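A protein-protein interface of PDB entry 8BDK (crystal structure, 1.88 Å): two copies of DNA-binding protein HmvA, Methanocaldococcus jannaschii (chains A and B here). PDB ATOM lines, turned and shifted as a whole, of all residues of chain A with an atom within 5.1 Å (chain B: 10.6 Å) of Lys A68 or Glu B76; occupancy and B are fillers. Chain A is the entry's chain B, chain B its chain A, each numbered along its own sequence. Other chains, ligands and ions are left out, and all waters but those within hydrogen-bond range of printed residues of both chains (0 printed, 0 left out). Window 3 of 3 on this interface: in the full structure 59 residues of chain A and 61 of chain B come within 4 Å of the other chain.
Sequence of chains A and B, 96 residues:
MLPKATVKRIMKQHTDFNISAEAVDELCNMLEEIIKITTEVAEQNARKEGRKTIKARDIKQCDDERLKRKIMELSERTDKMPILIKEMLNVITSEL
Among the printed residues, merely in contact across the chains: Asp A64 with Thr B78, Leu A67 with Thr B78, Leu A67 with Lys B86, Lys A68 with Ser B75, Lys A70 with Asn B90, Ile A71 with Ile B71, Ile A71 with Ser B75, Ile A71 with Leu B89 and Met A72 with Met B72.
Of the 19 printed residues of chain B, 10 touch a printed residue of chain A.
Hydrophobic or aromatic side chains of chain B that line the printed part of chain A: Ile B71, Met B72 and Leu B89.
Of the 10 printed residues of chain A, 6 touch a printed residue of chain B.
Hydrophobic or aromatic side chains of chain A that line the printed part of chain B: Leu A67, Ile A71 and Met A72.
Among the printed residues, Asp or Glu carboxylates within 4 Å of a Lys or Arg side-chain nitrogen of the other chain: Asp A64 with Lys B86 (2.5 Å) and Lys A68 with Glu B76 (3.9 Å).
O of Asn B90 lies within hydrogen-bond range of OG1 of Thr B93 (3.2 Å).
O of Met B72 is in hydrogen-bond range of OG of Ser B75 (2.5 Å).
The side-chain hydroxyl of Thr B93 lies within hydrogen-bond range of the backbone carbonyl oxygen of Leu B89 (2.8 Å).
Ile B71 touches its own counterpart, Ile A71.
Met B72 touches its own counterpart, Met A72.
Positions printed for both chains: 68, 69, 70, 71 and 72.
Of the 14 pairs that touch across the chains among the printed residues, 2 have their exchanged pair printed and touching as well.
Glu B76 touches just one residue of chain A: Lys A68 (3.7 Å).
Printed residues of chain B within 4 Å of Leu A67: Thr B78 (3.7 Å) and Lys B86 (3.9 Å).
Ile A71 touches three residues of chain B.
Of the printed residues of chain A, Thr B78 touches Asp A64 (3.6 Å) and Leu A67 (3.7 Å).
Printed residues of chain A within 4 Å of Ser B75: Lys A68 (3.3 Å), Ile A71 (3.6 Å) and Met A72 (3.2 Å).
Of the printed residues of chain A, Thr B93 touches Lys A70.
Printed residues of chain A within 4 Å of Ile B71: Ile A71 (3.3 Å).
Printed residues of chain A within 4 Å of Lys B86: Asp A64 (2.5 Å) and Leu A67 (3.9 Å).
OG of Ser B75 sits at hydrogen-bond distance from SD of Met A72, at 3.2 Å.
The side-chain carboxylate (OD1) of Asp A64 lies within salt-bridge range of the side-chain amino group (NZ) of Lys B86, at 2.5 Å.
The side-chain carboxylate of Glu B76 lies within salt-bridge range of the side-chain amino group of Lys A68 (3.9 Å).
The side-chain carboxylate (OD1) of Asp B79 sits close to the side-chain carboxylate (OD2) of Asp A64.
OG1 of Thr B93 lies close to NZ of Lys A70 (3.3 Å).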
ATOM      1  N   ASP A  63      10.375   3.503  -2.978  1.00  0.00           N
ATOM      2  CA  ASP A  63      11.266   2.649  -3.744  1.00  0.00           C
ATOM      3  C   ASP A  63      10.449   1.837  -4.735  1.00  0.00           C
ATOM      4  O   ASP A  63       9.224   1.741  -4.639  1.00  0.00           O
ATOM      5  CB  ASP A  63      12.071   1.713  -2.831  1.00  0.00           C
ATOM      6  CG  ASP A  63      13.355   1.217  -3.480  1.00  0.00           C
ATOM      7  OD1 ASP A  63      13.482   1.331  -4.717  1.00  0.00           O
ATOM      8  OD2 ASP A  63      14.247   0.711  -2.758  1.00  0.00           O
ATOM      9  N   ASP A  64      11.150   1.253  -5.707  1.00  0.00           N
ATOM     10  CA  ASP A  64      10.534   0.217  -6.521  1.00  0.00           C
ATOM     11  C   ASP A  64      10.173  -1.003  -5.683  1.00  0.00           C
ATOM     12  O   ASP A  64       9.380  -1.838  -6.130  1.00  0.00           O
ATOM     13  CB  ASP A  64      11.466  -0.182  -7.672  1.00  0.00           C
ATOM     14  CG  ASP A  64      11.846   0.999  -8.563  1.00  0.00           C
ATOM     15  OD1 ASP A  64      11.040   1.947  -8.688  1.00  0.00           O
ATOM     16  OD2 ASP A  64      12.954   0.975  -9.144  1.00  0.00           O
ATOM     17  N   GLU A  65      10.733  -1.117  -4.474  1.00  0.00           N
ATOM     18  CA  GLU A  65      10.418  -2.237  -3.593  1.00  0.00           C
ATOM     19  C   GLU A  65       9.105  -2.010  -2.853  1.00  0.00           C
ATOM     20  O   GLU A  65       8.249  -2.900  -2.809  1.00  0.00           O
ATOM     21  CB  GLU A  65      11.560  -2.465  -2.598  1.00  0.00           C
ATOM     22  CG  GLU A  65      12.929  -2.651  -3.240  1.00  0.00           C
ATOM     23  CD  GLU A  65      13.003  -3.880  -4.129  1.00  0.00           C
ATOM     24  OE1 GLU A  65      12.263  -4.853  -3.873  1.00  0.00           O
ATOM     25  OE2 GLU A  65      13.802  -3.871  -5.090  1.00  0.00           O
ATOM     26  N   ARG A  66       8.928  -0.829  -2.258  1.00  0.00           N
ATOM     27  CA  ARG A  66       7.680  -0.556  -1.555  1.00  0.00           C
ATOM     28  C   ARG A  66       6.527  -0.375  -2.533  1.00  0.00           C
ATOM     29  O   ARG A  66       5.398  -0.793  -2.252  1.00  0.00           O
ATOM     30  CB  ARG A  66       7.819   0.683  -0.676  1.00  0.00           C
ATOM     31  CG  ARG A  66       6.912   0.641   0.535  1.00  0.00           C
ATOM     32  CD  ARG A  66       6.290   1.988   0.844  1.00  0.00           C
ATOM     33  NE  ARG A  66       6.058   2.137   2.278  1.00  0.00           N
ATOM     34  CZ  ARG A  66       5.043   1.583   2.936  1.00  0.00           C
ATOM     35  NH1 ARG A  66       4.155   0.840   2.290  1.00  0.00           N
ATOM     36  NH2 ARG A  66       4.918   1.773   4.244  1.00  0.00           N
ATOM     37  N   LEU A  67       6.794   0.255  -3.681  1.00  0.00           N
ATOM     38  CA  LEU A  67       5.760   0.420  -4.699  1.00  0.00           C
ATOM     39  C   LEU A  67       5.266  -0.930  -5.201  1.00  0.00           C
ATOM     40  O   LEU A  67       4.054  -1.151  -5.315  1.00  0.00           O
ATOM     41  CB  LEU A  67       6.291   1.261  -5.859  1.00  0.00           C
ATOM     42  CG  LEU A  67       5.278   1.514  -6.975  1.00  0.00           C
ATOM     43  CD1 LEU A  67       4.064   2.258  -6.437  1.00  0.00           C
ATOM     44  CD2 LEU A  67       5.912   2.276  -8.122  1.00  0.00           C
ATOM     45  N   LYS A  68       6.193  -1.845  -5.499  1.00  0.00           N
ATOM     46  CA  LYS A  68       5.824  -3.188  -5.938  1.00  0.00           C
ATOM     47  C   LYS A  68       4.908  -3.876  -4.930  1.00  0.00           C
ATOM     48  O   LYS A  68       3.947  -4.550  -5.315  1.00  0.00           O
ATOM     49  CB  LYS A  68       7.086  -4.019  -6.172  1.00  0.00           C
ATOM     50  CG  LYS A  68       6.835  -5.452  -6.609  1.00  0.00           C
ATOM     51  CD  LYS A  68       8.095  -6.297  -6.486  1.00  0.00           C
ATOM     52  CE  LYS A  68       7.821  -7.751  -6.848  1.00  0.00           C
ATOM     53  NZ  LYS A  68       8.936  -8.661  -6.458  1.00  0.00           N
ATOM     54  N   ARG A  69       5.186  -3.717  -3.635  1.00  0.00           N
ATOM     55  CA  ARG A  69       4.344  -4.342  -2.620  1.00  0.00           C
ATOM     56  C   ARG A  69       2.949  -3.726  -2.594  1.00  0.00           C
ATOM     57  O   ARG A  69       1.950  -4.442  -2.456  1.00  0.00           O
ATOM     58  CB  ARG A  69       5.006  -4.229  -1.251  1.00  0.00           C
ATOM     59  CG  ARG A  69       6.213  -5.132  -1.072  1.00  0.00           C
ATOM     60  CD  ARG A  69       6.882  -4.909   0.276  1.00  0.00           C
ATOM     61  NE  ARG A  69       5.956  -5.078   1.392  1.00  0.00           N
ATOM     62  CZ  ARG A  69       5.408  -4.077   2.076  1.00  0.00           C
ATOM     63  NH1 ARG A  69       5.693  -2.822   1.765  1.00  0.00           N
ATOM     64  NH2 ARG A  69       4.577  -4.335   3.075  1.00  0.00           N
ATOM     65  N   LYS A  70       2.859  -2.402  -2.722  1.00  0.00           N
ATOM     66  CA  LYS A  70       1.559  -1.744  -2.660  1.00  0.00           C
ATOM     67  C   LYS A  70       0.725  -2.022  -3.906  1.00  0.00           C
ATOM     68  O   LYS A  70      -0.509  -2.035  -3.831  1.00  0.00           O
ATOM     69  CB  LYS A  70       1.741  -0.235  -2.454  1.00  0.00           C
ATOM     70  CG  LYS A  70       2.429   0.137  -1.140  1.00  0.00           C
ATOM     71  CD  LYS A  70       2.026   1.532  -0.665  1.00  0.00           C
ATOM     72  CE  LYS A  70       2.577   2.634  -1.570  1.00  0.00           C
ATOM     73  NZ  LYS A  70       2.025   3.984  -1.238  1.00  0.00           N
ATOM     74  N   ILE A  71       1.377  -2.239  -5.052  1.00  0.00           N
ATOM     75  CA  ILE A  71       0.657  -2.580  -6.273  1.00  0.00           C
ATOM     76  C   ILE A  71       0.102  -3.996  -6.178  1.00  0.00           C
ATOM     77  O   ILE A  71      -1.013  -4.275  -6.637  1.00  0.00           O
ATOM     78  CB  ILE A  71       1.575  -2.404  -7.497  1.00  0.00           C
ATOM     79  CG1 ILE A  71       1.960  -0.932  -7.675  1.00  0.00           C
ATOM     80  CG2 ILE A  71       0.914  -2.929  -8.766  1.00  0.00           C
ATOM     81  CD1 ILE A  71       2.944  -0.714  -8.783  1.00  0.00           C
ATOM     82  N   MET A  72       0.868  -4.907  -5.573  1.00  0.00           N
ATOM     83  CA  MET A  72       0.348  -6.236  -5.269  1.00  0.00           C
ATOM     84  C   MET A  72      -0.882  -6.146  -4.375  1.00  0.00           C
ATOM     85  O   MET A  72      -1.938  -6.703  -4.692  1.00  0.00           O
ATOM     86  CB  MET A  72       1.433  -7.083  -4.600  1.00  0.00           C
ATOM     87  CG  MET A  72       2.552  -7.526  -5.525  1.00  0.00           C
ATOM     88  SD  MET A  72       1.967  -8.693  -6.767  1.00  0.00           S
ATOM     89  CE  MET A  72       1.370 -10.019  -5.725  1.00  0.00           C
ATOM     90  N   LYS B  68      -7.600  -7.386 -11.743  1.00  0.00           N
ATOM     91  CA  LYS B  68      -6.753  -7.862 -10.655  1.00  0.00           C
ATOM     92  C   LYS B  68      -5.503  -8.554 -11.189  1.00  0.00           C
ATOM     93  O   LYS B  68      -4.410  -8.384 -10.639  1.00  0.00           O
ATOM     94  CB  LYS B  68      -7.563  -8.793  -9.755  1.00  0.00           C
ATOM     95  CG  LYS B  68      -6.796  -9.460  -8.641  1.00  0.00           C
ATOM     96  CD  LYS B  68      -7.741  -9.866  -7.521  1.00  0.00           C
ATOM     97  CE  LYS B  68      -8.799 -10.836  -7.993  1.00  0.00           C
ATOM     98  NZ  LYS B  68      -8.243 -12.203  -8.153  1.00  0.00           N
ATOM     99  N   ARG B  69      -5.642  -9.349 -12.255  1.00  0.00           N
ATOM    100  CA  ARG B  69      -4.462  -9.914 -12.903  1.00  0.00           C
ATOM    101  C   ARG B  69      -3.611  -8.825 -13.545  1.00  0.00           C
ATOM    102  O   ARG B  69      -2.380  -8.871 -13.473  1.00  0.00           O
ATOM    103  CB  ARG B  69      -4.875 -10.944 -13.952  1.00  0.00           C
ATOM    104  CG  ARG B  69      -3.722 -11.462 -14.817  1.00  0.00           C
ATOM    105  CD  ARG B  69      -4.218 -12.347 -15.981  1.00  0.00           C
ATOM    106  NE  ARG B  69      -5.229 -11.660 -16.784  1.00  0.00           N
ATOM    107  CZ  ARG B  69      -4.964 -10.770 -17.740  1.00  0.00           C
ATOM    108  NH1 ARG B  69      -3.707 -10.451 -18.039  1.00  0.00           N
ATOM    109  NH2 ARG B  69      -5.963 -10.192 -18.398  1.00  0.00           N
ATOM    110  N   LYS B  70      -4.253  -7.845 -14.186  1.00  0.00           N
ATOM    111  CA  LYS B  70      -3.526  -6.817 -14.914  1.00  0.00           C
ATOM    112  C   LYS B  70      -2.728  -5.937 -13.970  1.00  0.00           C
ATOM    113  O   LYS B  70      -1.651  -5.452 -14.334  1.00  0.00           O
ATOM    114  CB  LYS B  70      -4.501  -5.973 -15.736  1.00  0.00           C
ATOM    115  CG  LYS B  70      -4.998  -6.661 -17.003  1.00  0.00           C
ATOM    116  CD  LYS B  70      -6.262  -6.000 -17.532  1.00  0.00           C
ATOM    117  CE  LYS B  70      -5.982  -4.647 -18.166  1.00  0.00           C
ATOM    118  NZ  LYS B  70      -5.215  -4.803 -19.433  1.00  0.00           N
ATOM    119  N   ILE B  71      -3.237  -5.730 -12.755  1.00  0.00           N
ATOM    120  CA  ILE B  71      -2.488  -4.986 -11.748  1.00  0.00           C
ATOM    121  C   ILE B  71      -1.341  -5.834 -11.210  1.00  0.00           C
ATOM    122  O   ILE B  71      -0.209  -5.352 -11.060  1.00  0.00           O
ATOM    123  CB  ILE B  71      -3.430  -4.512 -10.629  1.00  0.00           C
ATOM    124  CG1 ILE B  71      -4.383  -3.442 -11.170  1.00  0.00           C
ATOM    125  CG2 ILE B  71      -2.643  -3.980  -9.457  1.00  0.00           C
ATOM    126  CD1 ILE B  71      -5.538  -3.136 -10.226  1.00  0.00           C
ATOM    127  N   MET B  72      -1.609  -7.111 -10.934  1.00  0.00           N
ATOM    128  CA  MET B  72      -0.563  -7.993 -10.431  1.00  0.00           C
ATOM    129  C   MET B  72       0.591  -8.097 -11.421  1.00  0.00           C
ATOM    130  O   MET B  72       1.761  -8.084 -11.026  1.00  0.00           O
ATOM    131  CB  MET B  72      -1.149  -9.377 -10.123  1.00  0.00           C
ATOM    132  CG  MET B  72      -0.740  -9.943  -8.776  1.00  0.00           C
ATOM    133  SD  MET B  72      -1.847 -11.213  -8.119  1.00  0.00           S
ATOM    134  CE  MET B  72      -2.476 -11.965  -9.617  1.00  0.00           C
ATOM    135  N   GLU B  73       0.282  -8.220 -12.712  1.00  0.00           N
ATOM    136  CA  GLU B  73       1.340  -8.256 -13.717  1.00  0.00           C
ATOM    137  C   GLU B  73       2.086  -6.929 -13.784  1.00  0.00           C
ATOM    138  O   GLU B  73       3.307  -6.904 -13.985  1.00  0.00           O
ATOM    139  CB  GLU B  73       0.752  -8.616 -15.079  1.00  0.00           C
ATOM    140  CG  GLU B  73       0.124  -9.998 -15.120  1.00  0.00           C
ATOM    141  CD  GLU B  73      -0.514 -10.304 -16.454  1.00  0.00           C
ATOM    142  OE1 GLU B  73      -1.027  -9.357 -17.091  1.00  0.00           O
ATOM    143  OE2 GLU B  73      -0.501 -11.486 -16.866  1.00  0.00           O
ATOM    144  N   LEU B  74       1.365  -5.817 -13.612  1.00  0.00           N
ATOM    145  CA  LEU B  74       1.997  -4.502 -13.598  1.00  0.00           C
ATOM    146  C   LEU B  74       2.986  -4.370 -12.451  1.00  0.00           C
ATOM    147  O   LEU B  74       3.971  -3.626 -12.562  1.00  0.00           O
ATOM    148  CB  LEU B  74       0.926  -3.414 -13.506  1.00  0.00           C
ATOM    149  CG  LEU B  74       1.333  -1.943 -13.343  1.00  0.00           C
ATOM    150  CD1 LEU B  74       1.957  -1.409 -14.619  1.00  0.00           C
ATOM    151  CD2 LEU B  74       0.137  -1.087 -12.927  1.00  0.00           C
ATOM    152  N   SER B  75       2.749  -5.089 -11.347  1.00  0.00           N
ATOM    153  CA  SER B  75       3.623  -4.985 -10.183  1.00  0.00           C
ATOM    154  C   SER B  75       5.050  -5.398 -10.497  1.00  0.00           C
ATOM    155  O   SER B  75       5.957  -5.089  -9.719  1.00  0.00           O
ATOM    156  CB  SER B  75       3.091  -5.840  -9.030  1.00  0.00           C
ATOM    157  OG  SER B  75       3.283  -7.220  -9.283  1.00  0.00           O
ATOM    158  N   GLU B  76       5.271  -6.079 -11.620  1.00  0.00           N
ATOM    159  CA  GLU B  76       6.600  -6.537 -11.997  1.00  0.00           C
ATOM    160  C   GLU B  76       7.098  -5.868 -13.276  1.00  0.00           C
ATOM    161  O   GLU B  76       7.976  -6.409 -13.952  1.00  0.00           O
ATOM    162  CB  GLU B  76       6.602  -8.061 -12.134  1.00  0.00           C
ATOM    163  CG  GLU B  76       5.814  -8.776 -11.033  1.00  0.00           C
ATOM    164  CD  GLU B  76       6.695  -9.548 -10.070  1.00  0.00           C
ATOM    165  OE1 GLU B  76       6.144 -10.295  -9.234  1.00  0.00           O
ATOM    166  OE2 GLU B  76       7.935  -9.416 -10.149  1.00  0.00           O
ATOM    167  N   ARG B  77       6.556  -4.702 -13.626  1.00  0.00           N
ATOM    168  CA  ARG B  77       7.124  -3.860 -14.673  1.00  0.00           C
ATOM    169  C   ARG B  77       7.487  -2.480 -14.126  1.00  0.00           C
ATOM    170  O   ARG B  77       7.457  -1.490 -14.856  1.00  0.00           O
ATOM    171  CB  ARG B  77       6.171  -3.730 -15.864  1.00  0.00           C
ATOM    172  CG  ARG B  77       5.736  -5.057 -16.494  1.00  0.00           C
ATOM    173  CD  ARG B  77       5.047  -4.865 -17.865  1.00  0.00           C
ATOM    174  NE  ARG B  77       3.740  -4.197 -17.803  1.00  0.00           N
ATOM    175  CZ  ARG B  77       2.568  -4.834 -17.805  1.00  0.00           C
ATOM    176  NH1 ARG B  77       2.528  -6.160 -17.855  1.00  0.00           N
ATOM    177  NH2 ARG B  77       1.429  -4.146 -17.753  1.00  0.00           N
ATOM    178  N   THR B  78       7.851  -2.408 -12.840  1.00  0.00           N
ATOM    179  CA  THR B  78       8.081  -1.131 -12.171  1.00  0.00           C
ATOM    180  C   THR B  78       9.459  -0.547 -12.475  1.00  0.00           C
ATOM    181  O   THR B  78       9.616   0.680 -12.516  1.00  0.00           O
ATOM    182  CB  THR B  78       7.902  -1.302 -10.655  1.00  0.00           C
ATOM    183  OG1 THR B  78       6.553  -1.676 -10.365  1.00  0.00           O
ATOM    184  CG2 THR B  78       8.220  -0.016  -9.909  1.00  0.00           C
ATOM    185  N   ASP B  79      10.468  -1.389 -12.699  1.00  0.00           N
ATOM    186  CA  ASP B  79      11.832  -0.876 -12.789  1.00  0.00           C
ATOM    187  C   ASP B  79      12.064  -0.011 -14.025  1.00  0.00           C
ATOM    188  O   ASP B  79      12.969   0.831 -14.013  1.00  0.00           O
ATOM    189  CB  ASP B  79      12.827  -2.036 -12.741  1.00  0.00           C
ATOM    190  CG  ASP B  79      12.921  -2.655 -11.357  1.00  0.00           C
ATOM    191  OD1 ASP B  79      12.735  -1.917 -10.363  1.00  0.00           O
ATOM    192  OD2 ASP B  79      13.169  -3.876 -11.259  1.00  0.00           O
ATOM    193  N   LYS B  80      11.267  -0.178 -15.080  1.00  0.00           N
ATOM    194  CA  LYS B  80      11.356   0.675 -16.258  1.00  0.00           C
ATOM    195  C   LYS B  80      10.129   1.562 -16.406  1.00  0.00           C
ATOM    196  O   LYS B  80       9.906   2.150 -17.468  1.00  0.00           O
ATOM    197  CB  LYS B  80      11.570  -0.174 -17.510  1.00  0.00           C
ATOM    198  CG  LYS B  80      12.979  -0.749 -17.598  1.00  0.00           C
ATOM    199  CD  LYS B  80      13.198  -1.474 -18.912  1.00  0.00           C
ATOM    200  CE  LYS B  80      14.579  -2.074 -18.962  1.00  0.00           C
ATOM    201  NZ  LYS B  80      14.843  -2.676 -20.284  1.00  0.00           N
ATOM    202  N   MET B  81       9.354   1.684 -15.349  1.00  0.00           N
ATOM    203  CA  MET B  81       8.115   2.453 -15.321  1.00  0.00           C
ATOM    204  C   MET B  81       8.407   3.952 -15.257  1.00  0.00           C
ATOM    205  O   MET B  81       9.238   4.381 -14.447  1.00  0.00           O
ATOM    206  CB  MET B  81       7.293   2.006 -14.121  1.00  0.00           C
ATOM    207  CG  MET B  81       6.006   2.727 -13.883  1.00  0.00           C
ATOM    208  SD  MET B  81       5.176   1.936 -12.488  1.00  0.00           S
ATOM    209  CE  MET B  81       4.642   0.406 -13.251  1.00  0.00           C
ATOM    210  N   ILE B  85       4.235   7.815 -13.896  1.00  0.00           N
ATOM    211  CA  ILE B  85       3.325   6.702 -13.644  1.00  0.00           C
ATOM    212  C   ILE B  85       3.537   6.135 -12.245  1.00  0.00           C
ATOM    213  O   ILE B  85       2.575   5.797 -11.561  1.00  0.00           O
ATOM    214  CB  ILE B  85       3.485   5.610 -14.718  1.00  0.00           C
ATOM    215  CG1 ILE B  85       3.032   6.127 -16.088  1.00  0.00           C
ATOM    216  CG2 ILE B  85       2.709   4.354 -14.317  1.00  0.00           C
ATOM    217  CD1 ILE B  85       1.553   6.450 -16.163  1.00  0.00           C
ATOM    218  N   LYS B  86       4.799   5.996 -11.805  1.00  0.00           N
ATOM    219  CA  LYS B  86       5.049   5.578 -10.429  1.00  0.00           C
ATOM    220  C   LYS B  86       4.356   6.518  -9.448  1.00  0.00           C
ATOM    221  O   LYS B  86       3.808   6.076  -8.431  1.00  0.00           O
ATOM    222  CB  LYS B  86       6.552   5.553 -10.125  1.00  0.00           C
ATOM    223  CG  LYS B  86       7.400   4.541 -10.901  1.00  0.00           C
ATOM    224  CD  LYS B  86       8.854   4.559 -10.387  1.00  0.00           C
ATOM    225  CE  LYS B  86       9.796   3.696 -11.224  1.00  0.00           C
ATOM    226  NZ  LYS B  86      11.133   3.523 -10.567  1.00  0.00           N
ATOM    227  N   LEU B  89       0.653   5.819  -9.380  1.00  0.00           N
ATOM    228  CA  LEU B  89       0.390   4.579  -8.656  1.00  0.00           C
ATOM    229  C   LEU B  89       0.640   4.756  -7.171  1.00  0.00           C
ATOM    230  O   LEU B  89      -0.061   4.168  -6.340  1.00  0.00           O
ATOM    231  CB  LEU B  89       1.260   3.454  -9.217  1.00  0.00           C
ATOM    232  CG  LEU B  89       0.835   2.989 -10.610  1.00  0.00           C
ATOM    233  CD1 LEU B  89       1.738   1.880 -11.137  1.00  0.00           C
ATOM    234  CD2 LEU B  89      -0.607   2.511 -10.552  1.00  0.00           C
ATOM    235  N   ASN B  90       1.653   5.547  -6.821  1.00  0.00           N
ATOM    236  CA  ASN B  90       1.906   5.843  -5.415  1.00  0.00           C
ATOM    237  C   ASN B  90       0.697   6.515  -4.783  1.00  0.00           C
ATOM    238  O   ASN B  90       0.283   6.154  -3.674  1.00  0.00           O
ATOM    239  CB  ASN B  90       3.145   6.726  -5.291  1.00  0.00           C
ATOM    240  CG  ASN B  90       3.751   6.680  -3.915  1.00  0.00           C
ATOM    241  OD1 ASN B  90       3.372   7.450  -3.034  1.00  0.00           O
ATOM    242  ND2 ASN B  90       4.702   5.773  -3.717  1.00  0.00           N
ATOM    243  N   THR B  93      -2.236   3.912  -4.579  1.00  0.00           N
ATOM    244  CA  THR B  93      -2.055   2.919  -3.526  1.00  0.00           C
ATOM    245  C   THR B  93      -2.063   3.560  -2.146  1.00  0.00           C
ATOM    246  O   THR B  93      -2.524   2.933  -1.185  1.00  0.00           O
ATOM    247  CB  THR B  93      -0.773   2.114  -3.758  1.00  0.00           C
ATOM    248  OG1 THR B  93       0.355   2.992  -3.861  1.00  0.00           O
ATOM    249  CG2 THR B  93      -0.890   1.313  -5.035  1.00  0.00           C
